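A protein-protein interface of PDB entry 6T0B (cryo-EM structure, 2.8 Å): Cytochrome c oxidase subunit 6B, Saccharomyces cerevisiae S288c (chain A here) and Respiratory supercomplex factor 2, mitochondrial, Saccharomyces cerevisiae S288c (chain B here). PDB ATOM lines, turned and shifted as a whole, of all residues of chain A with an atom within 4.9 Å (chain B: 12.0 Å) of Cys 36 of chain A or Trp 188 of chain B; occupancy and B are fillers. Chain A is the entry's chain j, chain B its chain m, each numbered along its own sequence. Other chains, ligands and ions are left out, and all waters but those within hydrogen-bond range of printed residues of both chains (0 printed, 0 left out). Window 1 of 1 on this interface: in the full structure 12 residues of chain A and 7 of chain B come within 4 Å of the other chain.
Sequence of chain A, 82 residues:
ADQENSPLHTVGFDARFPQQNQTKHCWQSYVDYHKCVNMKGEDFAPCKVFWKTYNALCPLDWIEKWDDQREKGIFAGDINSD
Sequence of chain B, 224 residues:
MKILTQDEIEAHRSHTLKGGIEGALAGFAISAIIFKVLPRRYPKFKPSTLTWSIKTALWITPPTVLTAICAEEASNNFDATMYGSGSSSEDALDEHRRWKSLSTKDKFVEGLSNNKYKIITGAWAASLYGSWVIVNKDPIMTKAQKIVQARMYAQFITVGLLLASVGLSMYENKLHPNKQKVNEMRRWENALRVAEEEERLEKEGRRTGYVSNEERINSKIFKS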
ATOM      1  N   VAL A  31      16.178   3.263 -16.333  1.00  0.00           N
ATOM      2  CA  VAL A  31      14.974   3.958 -16.783  1.00  0.00           C
ATOM      3  C   VAL A  31      13.808   2.978 -16.858  1.00  0.00           C
ATOM      4  O   VAL A  31      12.657   3.354 -16.606  1.00  0.00           O
ATOM      5  CB  VAL A  31      15.214   4.709 -18.115  1.00  0.00           C
ATOM      6  CG1 VAL A  31      15.354   3.768 -19.295  1.00  0.00           C
ATOM      7  CG2 VAL A  31      14.103   5.720 -18.366  1.00  0.00           C
ATOM      8  N   ASP A  32      14.096   1.692 -17.072  1.00  0.00           N
ATOM      9  CA  ASP A  32      13.052   0.682 -17.063  1.00  0.00           C
ATOM     10  C   ASP A  32      12.552   0.422 -15.652  1.00  0.00           C
ATOM     11  O   ASP A  32      11.355   0.182 -15.450  1.00  0.00           O
ATOM     12  CB  ASP A  32      13.560  -0.606 -17.709  1.00  0.00           C
ATOM     13  CG  ASP A  32      13.633  -0.511 -19.226  1.00  0.00           C
ATOM     14  OD1 ASP A  32      13.284   0.558 -19.768  1.00  0.00           O
ATOM     15  OD2 ASP A  32      14.069  -1.491 -19.868  1.00  0.00           O
ATOM     16  N   TYR A  33      13.442   0.499 -14.658  1.00  0.00           N
ATOM     17  CA  TYR A  33      13.012   0.330 -13.276  1.00  0.00           C
ATOM     18  C   TYR A  33      12.190   1.516 -12.810  1.00  0.00           C
ATOM     19  O   TYR A  33      11.169   1.354 -12.134  1.00  0.00           O
ATOM     20  CB  TYR A  33      14.211   0.129 -12.354  1.00  0.00           C
ATOM     21  CG  TYR A  33      13.861   0.270 -10.888  1.00  0.00           C
ATOM     22  CD1 TYR A  33      13.219  -0.749 -10.212  1.00  0.00           C
ATOM     23  CD2 TYR A  33      14.187   1.416 -10.177  1.00  0.00           C
ATOM     24  CE1 TYR A  33      12.887  -0.630  -8.881  1.00  0.00           C
ATOM     25  CE2 TYR A  33      13.859   1.547  -8.850  1.00  0.00           C
ATOM     26  CZ  TYR A  33      13.213   0.520  -8.204  1.00  0.00           C
ATOM     27  OH  TYR A  33      12.895   0.655  -6.873  1.00  0.00           O
ATOM     28  N   HIS A  34      12.644   2.722 -13.117  1.00  0.00           N
ATOM     29  CA  HIS A  34      11.924   3.873 -12.606  1.00  0.00           C
ATOM     30  C   HIS A  34      10.678   4.195 -13.413  1.00  0.00           C
ATOM     31  O   HIS A  34       9.838   4.956 -12.930  1.00  0.00           O
ATOM     32  CB  HIS A  34      12.863   5.073 -12.521  1.00  0.00           C
ATOM     33  CG  HIS A  34      13.650   5.110 -11.254  1.00  0.00           C
ATOM     34  ND1 HIS A  34      14.889   4.521 -11.125  1.00  0.00           N
ATOM     35  CD2 HIS A  34      13.343   5.609 -10.037  1.00  0.00           C
ATOM     36  CE1 HIS A  34      15.320   4.680  -9.887  1.00  0.00           C
ATOM     37  NE2 HIS A  34      14.401   5.338  -9.206  1.00  0.00           N
ATOM     38  N   LYS A  35      10.519   3.631 -14.608  1.00  0.00           N
ATOM     39  CA  LYS A  35       9.252   3.696 -15.317  1.00  0.00           C
ATOM     40  C   LYS A  35       8.449   2.423 -15.165  1.00  0.00           C
ATOM     41  O   LYS A  35       7.385   2.274 -15.790  1.00  0.00           O
ATOM     42  CB  LYS A  35       9.510   4.047 -16.785  1.00  0.00           C
ATOM     43  CG  LYS A  35       9.704   2.984 -17.812  1.00  0.00           C
ATOM     44  CD  LYS A  35       9.620   3.508 -19.223  1.00  0.00           C
ATOM     45  CE  LYS A  35      10.938   4.100 -19.657  1.00  0.00           C
ATOM     46  NZ  LYS A  35      10.886   4.397 -21.110  1.00  0.00           N
ATOM     47  N   CYS A  36       8.929   1.482 -14.348  1.00  0.00           N
ATOM     48  CA  CYS A  36       7.978   0.534 -13.763  1.00  0.00           C
ATOM     49  C   CYS A  36       7.001   1.260 -12.848  1.00  0.00           C
ATOM     50  O   CYS A  36       5.805   1.379 -13.141  1.00  0.00           O
ATOM     51  CB  CYS A  36       8.653  -0.582 -12.955  1.00  0.00           C
ATOM     52  SG  CYS A  36       9.525  -1.887 -13.704  1.00  0.00           S
ATOM     53  N   VAL A  37       7.531   1.819 -11.752  1.00  0.00           N
ATOM     54  CA  VAL A  37       6.786   2.056 -10.528  1.00  0.00           C
ATOM     55  C   VAL A  37       5.744   3.154 -10.631  1.00  0.00           C
ATOM     56  O   VAL A  37       5.047   3.408  -9.643  1.00  0.00           O
ATOM     57  CB  VAL A  37       7.784   2.343  -9.385  1.00  0.00           C
ATOM     58  CG1 VAL A  37       8.674   1.134  -9.132  1.00  0.00           C
ATOM     59  CG2 VAL A  37       8.623   3.566  -9.666  1.00  0.00           C
ATOM     60  N   ASN A  38       5.599   3.790 -11.790  1.00  0.00           N
ATOM     61  CA  ASN A  38       4.423   4.593 -12.085  1.00  0.00           C
ATOM     62  C   ASN A  38       3.323   3.759 -12.730  1.00  0.00           C
ATOM     63  O   ASN A  38       2.148   3.899 -12.370  1.00  0.00           O
ATOM     64  CB  ASN A  38       4.797   5.766 -12.996  1.00  0.00           C
ATOM     65  CG  ASN A  38       5.540   5.322 -14.226  1.00  0.00           C
ATOM     66  OD1 ASN A  38       5.987   4.187 -14.286  1.00  0.00           O
ATOM     67  ND2 ASN A  38       5.664   6.200 -15.219  1.00  0.00           N
ATOM     68  N   MET A  39       3.693   2.891 -13.673  1.00  0.00           N
ATOM     69  CA  MET A  39       2.766   2.066 -14.433  1.00  0.00           C
ATOM     70  C   MET A  39       2.512   0.739 -13.753  1.00  0.00           C
ATOM     71  O   MET A  39       1.464   0.123 -13.968  1.00  0.00           O
ATOM     72  CB  MET A  39       3.326   1.807 -15.838  1.00  0.00           C
ATOM     73  CG  MET A  39       3.539   3.061 -16.667  1.00  0.00           C
ATOM     74  SD  MET A  39       4.384   2.634 -18.194  1.00  0.00           S
ATOM     75  CE  MET A  39       4.558   4.227 -18.994  1.00  0.00           C
ATOM     76  N   LYS A  40       3.463   0.320 -12.932  1.00  0.00           N
ATOM     77  CA  LYS A  40       3.519  -0.995 -12.309  1.00  0.00           C
ATOM     78  C   LYS A  40       3.145  -0.865 -10.863  1.00  0.00           C
ATOM     79  O   LYS A  40       2.239  -1.537 -10.369  1.00  0.00           O
ATOM     80  CB  LYS A  40       4.937  -1.558 -12.326  1.00  0.00           C
ATOM     81  CG  LYS A  40       5.354  -2.323 -13.541  1.00  0.00           C
ATOM     82  CD  LYS A  40       5.249  -1.491 -14.689  1.00  0.00           C
ATOM     83  CE  LYS A  40       5.973  -1.882 -15.761  1.00  0.00           C
ATOM     84  NZ  LYS A  40       5.295  -0.999 -16.754  1.00  0.00           N
ATOM     85  N   GLY A  41       3.901  -0.031 -10.180  1.00  0.00           N
ATOM     86  CA  GLY A  41       3.700   0.268  -8.795  1.00  0.00           C
ATOM     87  C   GLY A  41       4.718  -0.421  -7.915  1.00  0.00           C
ATOM     88  O   GLY A  41       5.729  -0.966  -8.362  1.00  0.00           O
ATOM     89  N   CYS A  47      10.307  -6.124 -11.348  1.00  0.00           N
ATOM     90  CA  CYS A  47      11.077  -4.911 -11.485  1.00  0.00           C
ATOM     91  C   CYS A  47      12.283  -4.916 -10.568  1.00  0.00           C
ATOM     92  O   CYS A  47      12.995  -3.915 -10.490  1.00  0.00           O
ATOM     93  CB  CYS A  47      10.188  -3.695 -11.257  1.00  0.00           C
ATOM     94  SG  CYS A  47      10.814  -2.276 -12.210  1.00  0.00           S
ATOM     95  N   PHE A  50      15.205  -5.478 -13.257  1.00  0.00           N
ATOM     96  CA  PHE A  50      15.816  -4.212 -13.645  1.00  0.00           C
ATOM     97  C   PHE A  50      16.721  -3.680 -12.548  1.00  0.00           C
ATOM     98  O   PHE A  50      17.791  -3.136 -12.833  1.00  0.00           O
ATOM     99  CB  PHE A  50      14.729  -3.198 -13.968  1.00  0.00           C
ATOM    100  CG  PHE A  50      13.923  -3.548 -15.169  1.00  0.00           C
ATOM    101  CD1 PHE A  50      14.543  -3.918 -16.344  1.00  0.00           C
ATOM    102  CD2 PHE A  50      12.542  -3.509 -15.125  1.00  0.00           C
ATOM    103  CE1 PHE A  50      13.803  -4.243 -17.457  1.00  0.00           C
ATOM    104  CE2 PHE A  50      11.798  -3.827 -16.236  1.00  0.00           C
ATOM    105  CZ  PHE A  50      12.429  -4.197 -17.402  1.00  0.00           C
ATOM    106  N   GLN B 180       7.098   8.917 -32.252  1.00  0.00           N
ATOM    107  CA  GLN B 180       8.273   9.250 -31.422  1.00  0.00           C
ATOM    108  C   GLN B 180       8.062   8.772 -29.989  1.00  0.00           C
ATOM    109  O   GLN B 180       8.986   8.911 -29.174  1.00  0.00           O
ATOM    110  CB  GLN B 180       8.670  10.738 -31.380  1.00  0.00           C
ATOM    111  CG  GLN B 180       9.086  11.310 -32.717  1.00  0.00           C
ATOM    112  CD  GLN B 180      10.384  10.716 -33.211  1.00  0.00           C
ATOM    113  OE1 GLN B 180      11.311  10.490 -32.433  1.00  0.00           O
ATOM    114  NE2 GLN B 180      10.460  10.455 -34.510  1.00  0.00           N
ATOM    115  N   LYS B 181       6.884   8.243 -29.636  1.00  0.00           N
ATOM    116  CA  LYS B 181       6.737   7.514 -28.377  1.00  0.00           C
ATOM    117  C   LYS B 181       5.905   6.234 -28.456  1.00  0.00           C
ATOM    118  O   LYS B 181       6.038   5.404 -27.552  1.00  0.00           O
ATOM    119  CB  LYS B 181       6.175   8.432 -27.270  1.00  0.00           C
ATOM    120  CG  LYS B 181       4.756   8.963 -27.454  1.00  0.00           C
ATOM    121  CD  LYS B 181       3.717   8.156 -26.682  1.00  0.00           C
ATOM    122  CE  LYS B 181       2.334   8.730 -26.870  1.00  0.00           C
ATOM    123  NZ  LYS B 181       1.295   7.871 -26.251  1.00  0.00           N
ATOM    124  N   VAL B 182       5.046   6.021 -29.460  1.00  0.00           N
ATOM    125  CA  VAL B 182       4.138   4.873 -29.397  1.00  0.00           C
ATOM    126  C   VAL B 182       4.784   3.577 -29.879  1.00  0.00           C
ATOM    127  O   VAL B 182       4.101   2.553 -29.990  1.00  0.00           O
ATOM    128  CB  VAL B 182       2.818   5.104 -30.166  1.00  0.00           C
ATOM    129  CG1 VAL B 182       1.890   6.056 -29.405  1.00  0.00           C
ATOM    130  CG2 VAL B 182       3.066   5.544 -31.592  1.00  0.00           C
ATOM    131  N   ASN B 183       6.087   3.583 -30.167  1.00  0.00           N
ATOM    132  CA  ASN B 183       6.827   2.329 -30.141  1.00  0.00           C
ATOM    133  C   ASN B 183       8.080   2.384 -29.265  1.00  0.00           C
ATOM    134  O   ASN B 183       8.751   1.362 -29.105  1.00  0.00           O
ATOM    135  CB  ASN B 183       7.136   1.811 -31.565  1.00  0.00           C
ATOM    136  CG  ASN B 183       7.895   2.795 -32.425  1.00  0.00           C
ATOM    137  OD1 ASN B 183       8.649   3.637 -31.941  1.00  0.00           O
ATOM    138  ND2 ASN B 183       7.685   2.696 -33.734  1.00  0.00           N
ATOM    139  N   GLU B 184       8.366   3.517 -28.618  1.00  0.00           N
ATOM    140  CA  GLU B 184       9.037   3.406 -27.327  1.00  0.00           C
ATOM    141  C   GLU B 184       8.137   2.669 -26.347  1.00  0.00           C
ATOM    142  O   GLU B 184       8.624   1.963 -25.461  1.00  0.00           O
ATOM    143  CB  GLU B 184       9.431   4.780 -26.786  1.00  0.00           C
ATOM    144  CG  GLU B 184      10.481   5.480 -27.624  1.00  0.00           C
ATOM    145  CD  GLU B 184      11.821   4.774 -27.607  1.00  0.00           C
ATOM    146  OE1 GLU B 184      12.174   4.184 -26.564  1.00  0.00           O
ATOM    147  OE2 GLU B 184      12.521   4.807 -28.639  1.00  0.00           O
ATOM    148  N   MET B 185       6.820   2.827 -26.520  1.00  0.00           N
ATOM    149  CA  MET B 185       5.806   1.896 -26.038  1.00  0.00           C
ATOM    150  C   MET B 185       6.121   0.433 -26.349  1.00  0.00           C
ATOM    151  O   MET B 185       6.069  -0.408 -25.452  1.00  0.00           O
ATOM    152  CB  MET B 185       4.464   2.275 -26.660  1.00  0.00           C
ATOM    153  CG  MET B 185       3.281   1.492 -26.141  1.00  0.00           C
ATOM    154  SD  MET B 185       2.892   1.888 -24.429  1.00  0.00           S
ATOM    155  CE  MET B 185       1.994   0.420 -23.943  1.00  0.00           C
ATOM    156  N   ARG B 186       6.442   0.109 -27.617  1.00  0.00           N
ATOM    157  CA  ARG B 186       6.780  -1.266 -28.019  1.00  0.00           C
ATOM    158  C   ARG B 186       8.010  -1.771 -27.292  1.00  0.00           C
ATOM    159  O   ARG B 186       7.999  -2.858 -26.689  1.00  0.00           O
ATOM    160  CB  ARG B 186       7.069  -1.321 -29.530  1.00  0.00           C
ATOM    161  CG  ARG B 186       7.377  -2.709 -30.176  1.00  0.00           C
ATOM    162  CD  ARG B 186       8.866  -3.211 -30.215  1.00  0.00           C
ATOM    163  NE  ARG B 186       9.832  -2.367 -30.917  1.00  0.00           N
ATOM    164  CZ  ARG B 186      11.152  -2.518 -30.805  1.00  0.00           C
ATOM    165  NH1 ARG B 186      11.639  -3.485 -30.039  1.00  0.00           N
ATOM    166  NH2 ARG B 186      11.988  -1.715 -31.457  1.00  0.00           N
ATOM    167  N   ARG B 187       9.087  -0.987 -27.382  1.00  0.00           N
ATOM    168  CA  ARG B 187      10.377  -1.346 -26.814  1.00  0.00           C
ATOM    169  C   ARG B 187      10.271  -1.534 -25.311  1.00  0.00           C
ATOM    170  O   ARG B 187      10.675  -2.573 -24.775  1.00  0.00           O
ATOM    171  CB  ARG B 187      11.394  -0.259 -27.152  1.00  0.00           C
ATOM    172  CG  ARG B 187      12.836  -0.639 -26.904  1.00  0.00           C
ATOM    173  CD  ARG B 187      13.615   0.523 -26.312  1.00  0.00           C
ATOM    174  NE  ARG B 187      12.964   1.078 -25.130  1.00  0.00           N
ATOM    175  CZ  ARG B 187      13.086   0.575 -23.907  1.00  0.00           C
ATOM    176  NH1 ARG B 187      13.837  -0.497 -23.699  1.00  0.00           N
ATOM    177  NH2 ARG B 187      12.465   1.149 -22.887  1.00  0.00           N
ATOM    178  N   TRP B 188       9.635  -0.578 -24.626  1.00  0.00           N
ATOM    179  CA  TRP B 188       9.502  -0.661 -23.178  1.00  0.00           C
ATOM    180  C   TRP B 188       8.499  -1.729 -22.749  1.00  0.00           C
ATOM    181  O   TRP B 188       8.731  -2.400 -21.740  1.00  0.00           O
ATOM    182  CB  TRP B 188       9.125   0.719 -22.632  1.00  0.00           C
ATOM    183  CG  TRP B 188       8.384   0.717 -21.359  1.00  0.00           C
ATOM    184  CD1 TRP B 188       7.094   1.170 -21.155  1.00  0.00           C
ATOM    185  CD2 TRP B 188       8.820   0.181 -20.118  1.00  0.00           C
ATOM    186  NE1 TRP B 188       6.759   0.957 -19.872  1.00  0.00           N
ATOM    187  CE2 TRP B 188       7.802   0.359 -19.249  1.00  0.00           C
ATOM    188  CE3 TRP B 188       9.992  -0.405 -19.657  1.00  0.00           C
ATOM    189  CZ2 TRP B 188       7.945   0.040 -17.906  1.00  0.00           C
ATOM    190  CZ3 TRP B 188      10.077  -0.820 -18.368  1.00  0.00           C
ATOM    191  CH2 TRP B 188       9.062  -0.621 -17.519  1.00  0.00           C
ATOM    192  N   GLU B 189       7.455  -1.983 -23.547  1.00  0.00           N
ATOM    193  CA  GLU B 189       6.439  -2.977 -23.201  1.00  0.00           C
ATOM    194  C   GLU B 189       7.005  -4.395 -23.238  1.00  0.00           C
ATOM    195  O   GLU B 189       6.804  -5.200 -22.307  1.00  0.00           O
ATOM    196  CB  GLU B 189       5.254  -2.835 -24.160  1.00  0.00           C
ATOM    197  CG  GLU B 189       3.916  -3.288 -23.626  1.00  0.00           C
ATOM    198  CD  GLU B 189       3.709  -4.778 -23.791  1.00  0.00           C
ATOM    199  OE1 GLU B 189       3.172  -5.414 -22.859  1.00  0.00           O
ATOM    200  OE2 GLU B 189       4.095  -5.314 -24.852  1.00  0.00           O
ATOM    201  N   ASN B 190       7.753  -4.724 -24.284  1.00  0.00           N
ATOM    202  CA  ASN B 190       8.291  -6.074 -24.248  1.00  0.00           C
ATOM    203  C   ASN B 190       9.622  -6.182 -23.513  1.00  0.00           C
ATOM    204  O   ASN B 190       9.966  -7.291 -23.092  1.00  0.00           O
ATOM    205  CB  ASN B 190       8.398  -6.685 -25.645  1.00  0.00           C
ATOM    206  CG  ASN B 190       7.996  -8.162 -25.639  1.00  0.00           C
ATOM    207  OD1 ASN B 190       7.869  -8.764 -24.571  1.00  0.00           O
ATOM    208  ND2 ASN B 190       7.765  -8.736 -26.813  1.00  0.00           N
ATOM    209  N   ALA B 191      10.337  -5.077 -23.256  1.00  0.00           N
ATOM    210  CA  ALA B 191      11.473  -5.154 -22.338  1.00  0.00           C
ATOM    211  C   ALA B 191      10.994  -5.410 -20.912  1.00  0.00           C
ATOM    212  O   ALA B 191      11.620  -6.162 -20.140  1.00  0.00           O
ATOM    213  CB  ALA B 191      12.290  -3.865 -22.421  1.00  0.00           C
ATOM    214  N   LEU B 192       9.860  -4.803 -20.574  1.00  0.00           N
ATOM    215  CA  LEU B 192       9.109  -5.110 -19.367  1.00  0.00           C
ATOM    216  C   LEU B 192       8.810  -6.592 -19.243  1.00  0.00           C
ATOM    217  O   LEU B 192       9.394  -7.291 -18.410  1.00  0.00           O
ATOM    218  CB  LEU B 192       7.823  -4.312 -19.471  1.00  0.00           C
ATOM    219  CG  LEU B 192       6.724  -3.829 -18.575  1.00  0.00           C
ATOM    220  CD1 LEU B 192       5.938  -2.730 -19.326  1.00  0.00           C
ATOM    221  CD2 LEU B 192       5.780  -4.890 -18.007  1.00  0.00           C
ATOM    222  N   ARG B 193       7.989  -7.136 -20.124  1.00  0.00           N
ATOM    223  CA  ARG B 193       7.664  -8.542 -19.813  1.00  0.00           C
ATOM    224  C   ARG B 193       8.709  -9.569 -20.320  1.00  0.00           C
ATOM    225  O   ARG B 193       8.558 -10.756 -20.014  1.00  0.00           O
ATOM    226  CB  ARG B 193       6.251  -8.865 -20.225  1.00  0.00           C
ATOM    227  CG  ARG B 193       5.256  -8.233 -19.190  1.00  0.00           C
ATOM    228  CD  ARG B 193       3.790  -8.631 -19.330  1.00  0.00           C
ATOM    229  NE  ARG B 193       3.133  -8.034 -18.180  1.00  0.00           N
ATOM    230  CZ  ARG B 193       2.456  -6.893 -18.208  1.00  0.00           C
ATOM    231  NH1 ARG B 193       2.334  -6.231 -19.355  1.00  0.00           N
ATOM    232  NH2 ARG B 193       1.912  -6.408 -17.087  1.00  0.00           N
ATOM    233  N   VAL B 194       9.850  -9.124 -20.870  1.00  0.00           N
ATOM    234  CA  VAL B 194      10.984 -10.014 -20.887  1.00  0.00           C
ATOM    235  C   VAL B 194      11.724  -9.955 -19.548  1.00  0.00           C
ATOM    236  O   VAL B 194      12.444 -10.899 -19.227  1.00  0.00           O
ATOM    237  CB  VAL B 194      11.948  -9.737 -22.067  1.00  0.00           C
ATOM    238  CG1 VAL B 194      12.844  -8.550 -21.833  1.00  0.00           C
ATOM    239  CG2 VAL B 194      12.795 -10.970 -22.393  1.00  0.00           C
ATOM    240  N   ALA B 195      11.542  -8.920 -18.717  1.00  0.00           N
ATOM    241  CA  ALA B 195      11.925  -9.114 -17.315  1.00  0.00           C
ATOM    242  C   ALA B 195      10.986 -10.106 -16.624  1.00  0.00           C
ATOM    243  O   ALA B 195      11.404 -10.846 -15.712  1.00  0.00           O
ATOM    244  CB  ALA B 195      11.965  -7.789 -16.565  1.00  0.00           C
ATOM    245  N   GLU B 196       9.715 -10.119 -17.041  1.00  0.00           N
ATOM    246  CA  GLU B 196       8.756 -11.103 -16.506  1.00  0.00           C
ATOM    247  C   GLU B 196       9.138 -12.552 -16.833  1.00  0.00           C
ATOM    248  O   GLU B 196       9.043 -13.456 -15.985  1.00  0.00           O
ATOM    249  CB  GLU B 196       7.349 -10.809 -17.000  1.00  0.00           C
ATOM    250  CG  GLU B 196       6.482  -9.874 -16.154  1.00  0.00           C
ATOM    251  CD  GLU B 196       6.801  -8.411 -16.110  1.00  0.00           C
ATOM    252  OE1 GLU B 196       7.947  -8.028 -16.246  1.00  0.00           O
ATOM    253  OE2 GLU B 196       5.859  -7.591 -16.026  1.00  0.00           O
ATOM    254  N   GLU B 197       9.552 -12.806 -18.069  1.00  0.00           N
ATOM    255  CA  GLU B 197       9.953 -14.169 -18.438  1.00  0.00           C
ATOM    256  C   GLU B 197      11.162 -14.668 -17.644  1.00  0.00           C
ATOM    257  O   GLU B 197      11.303 -15.878 -17.435  1.00  0.00           O
ATOM    258  CB  GLU B 197      10.228 -14.263 -19.940  1.00  0.00           C
ATOM    259  CG  GLU B 197       8.996 -14.052 -20.772  1.00  0.00           C
ATOM    260  CD  GLU B 197       7.934 -15.126 -20.548  1.00  0.00           C
ATOM    261  OE1 GLU B 197       8.282 -16.299 -20.294  1.00  0.00           O
ATOM    262  OE2 GLU B 197       6.741 -14.768 -20.587  1.00  0.00           O
ATOM    263  N   GLU B 198      12.023 -13.766 -17.174  1.00  0.00           N
ATOM    264  CA  GLU B 198      13.121 -14.197 -16.320  1.00  0.00           C
ATOM    265  C   GLU B 198      12.679 -14.370 -14.869  1.00  0.00           C
ATOM    266  O   GLU B 198      13.108 -15.350 -14.230  1.00  0.00           O
ATOM    267  CB  GLU B 198      14.298 -13.229 -16.435  1.00  0.00           C
ATOM    268  CG  GLU B 198      14.602 -12.863 -17.880  1.00  0.00           C
ATOM    269  CD  GLU B 198      15.963 -12.231 -18.081  1.00  0.00           C
ATOM    270  OE1 GLU B 198      16.939 -12.984 -18.271  1.00  0.00           O
ATOM    271  OE2 GLU B 198      16.054 -10.985 -18.074  1.00  0.00           O
ATOM    272  N   GLU B 199      11.810 -13.456 -14.341  1.00  0.00           N
ATOM    273  CA  GLU B 199      11.432 -13.514 -12.914  1.00  0.00           C
ATOM    274  C   GLU B 199      10.751 -14.838 -12.574  1.00  0.00           C
ATOM    275  O   GLU B 199      10.939 -15.374 -11.469  1.00  0.00           O
ATOM    276  CB  GLU B 199      10.481 -12.372 -12.452  1.00  0.00           C
ATOM    277  CG  GLU B 199       9.072 -12.409 -13.197  1.00  0.00           C
ATOM    278  CD  GLU B 199       7.812 -11.915 -12.492  1.00  0.00           C
ATOM    279  OE1 GLU B 199       7.881 -11.715 -11.252  1.00  0.00           O
ATOM    280  OE2 GLU B 199       6.726 -11.802 -13.139  1.00  0.00           O
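The side-chain carboxylate (OD1) of Asp 32 of chain A is in salt-bridge range of the guanidinium group (NH2) of Arg 187 of chain B, 3.3 Å away.
The indole nitrogen (NE1) of Trp 188 of chain B sits at hydrogen-bond distance from the side-chain sulfur (SD) of Met 39 of chain A.
Of the 20 printed residues of chain B, 5 touch a printed residue of chain A.
Hydrophobic or aromatic side chains of chain A that line the printed part of chain B: Met 39 and Phe 50.
Along chain A the printed residues that touch a printed residue of chain B span positions 32 to 50.
No residue of chain B comes within 4 Å of Val 31 of chain A.
Asp 32 of chain A touches just these residues of chain B: Arg 187, Trp 188 and Ala 191.
No residue of chain B comes within 4 Å of Tyr 33 of chain A.
Cys 36 of chain A touches just one residue of chain B: Trp 188.
No residue of chain B comes within 4 Å of Val 37 of chain A.
Asn 38 of chain A touches none of the printed residues of chain B.
Of the printed residues of chain B, Met 39 of chain A touches Trp 188 (3.4 Å).
Of chain B, only Trp 188 and Leu 192 come within 4 Å of Lys 40 of chain A.
No residue of chain B comes within 4 Å of Gly 41 of chain A.
No residue of chain B comes within 4 Å of Cys 47 of chain A.
Arg 186 of chain B touches none of the printed residues of chain A.
Of the printed residues of chain A, Arg 187 of chain B touches Asp 32.
Of the printed residues of chain A, Trp 188 of chain B touches Asp 32 (3.2 Å), Lys 35 (3.1 Å), Cys 36 (3.8 Å), Met 39 (3.4 Å) and Lys 40 (3.1 Å).
Of the printed residues of chain A, Leu 192 of chain B touches Lys 40 (3.2 Å) and Phe 50 (3.96 Å).
Of the printed residues of chain A, Ala 195 of chain B touches Phe 50.
Among the printed residues, pairs that only touch across the chains: Lys 40 of chain A with Trp 188 of chain B (3.1 Å), Lys 35 of chain A with Trp 188 of chain B (3.1 Å), Lys 40 of chain A with Leu 192 of chain B (3.2 Å), Asp 32 of chain A with Trp 188 of chain B (3.2 Å), Phe 50 of chain A with Ala 191 of chain B (3.5 Å), Phe 50 of chain A with Ala 195 of chain B (3.7 Å), Cys 36 of chain A with Trp 188 of chain B (3.8 Å), Asp 32 of chain A with Ala 191 of chain B (3.9 Å) and Phe 50 of chain A with Leu 192 of chain B (3.96 Å).
OE1 of Glu 184 of chain B lies within salt-bridge range of NE of Arg 187 of chain B, at 3.5 Å.
OD1 of Asn 38 of chain A lies close to O of Lys 35 of chain A, 2.8 Å away.
SG of Cys 36 of chain A is disulfide-bonded to SG of Cys 47 of chain A, 2.0 Å away.
The backbone carbonyl oxygen (O) of Leu 192 of chain B sits close to the side-chain carboxylate (OE1) of Glu 196 of chain B, at 2.7 Å.
The backbone carbonyl oxygen (O) of Cys 36 of chain A sits close to the side-chain amide oxygen (OD1) of Asn 38 of chain A, 3.0 Å away.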
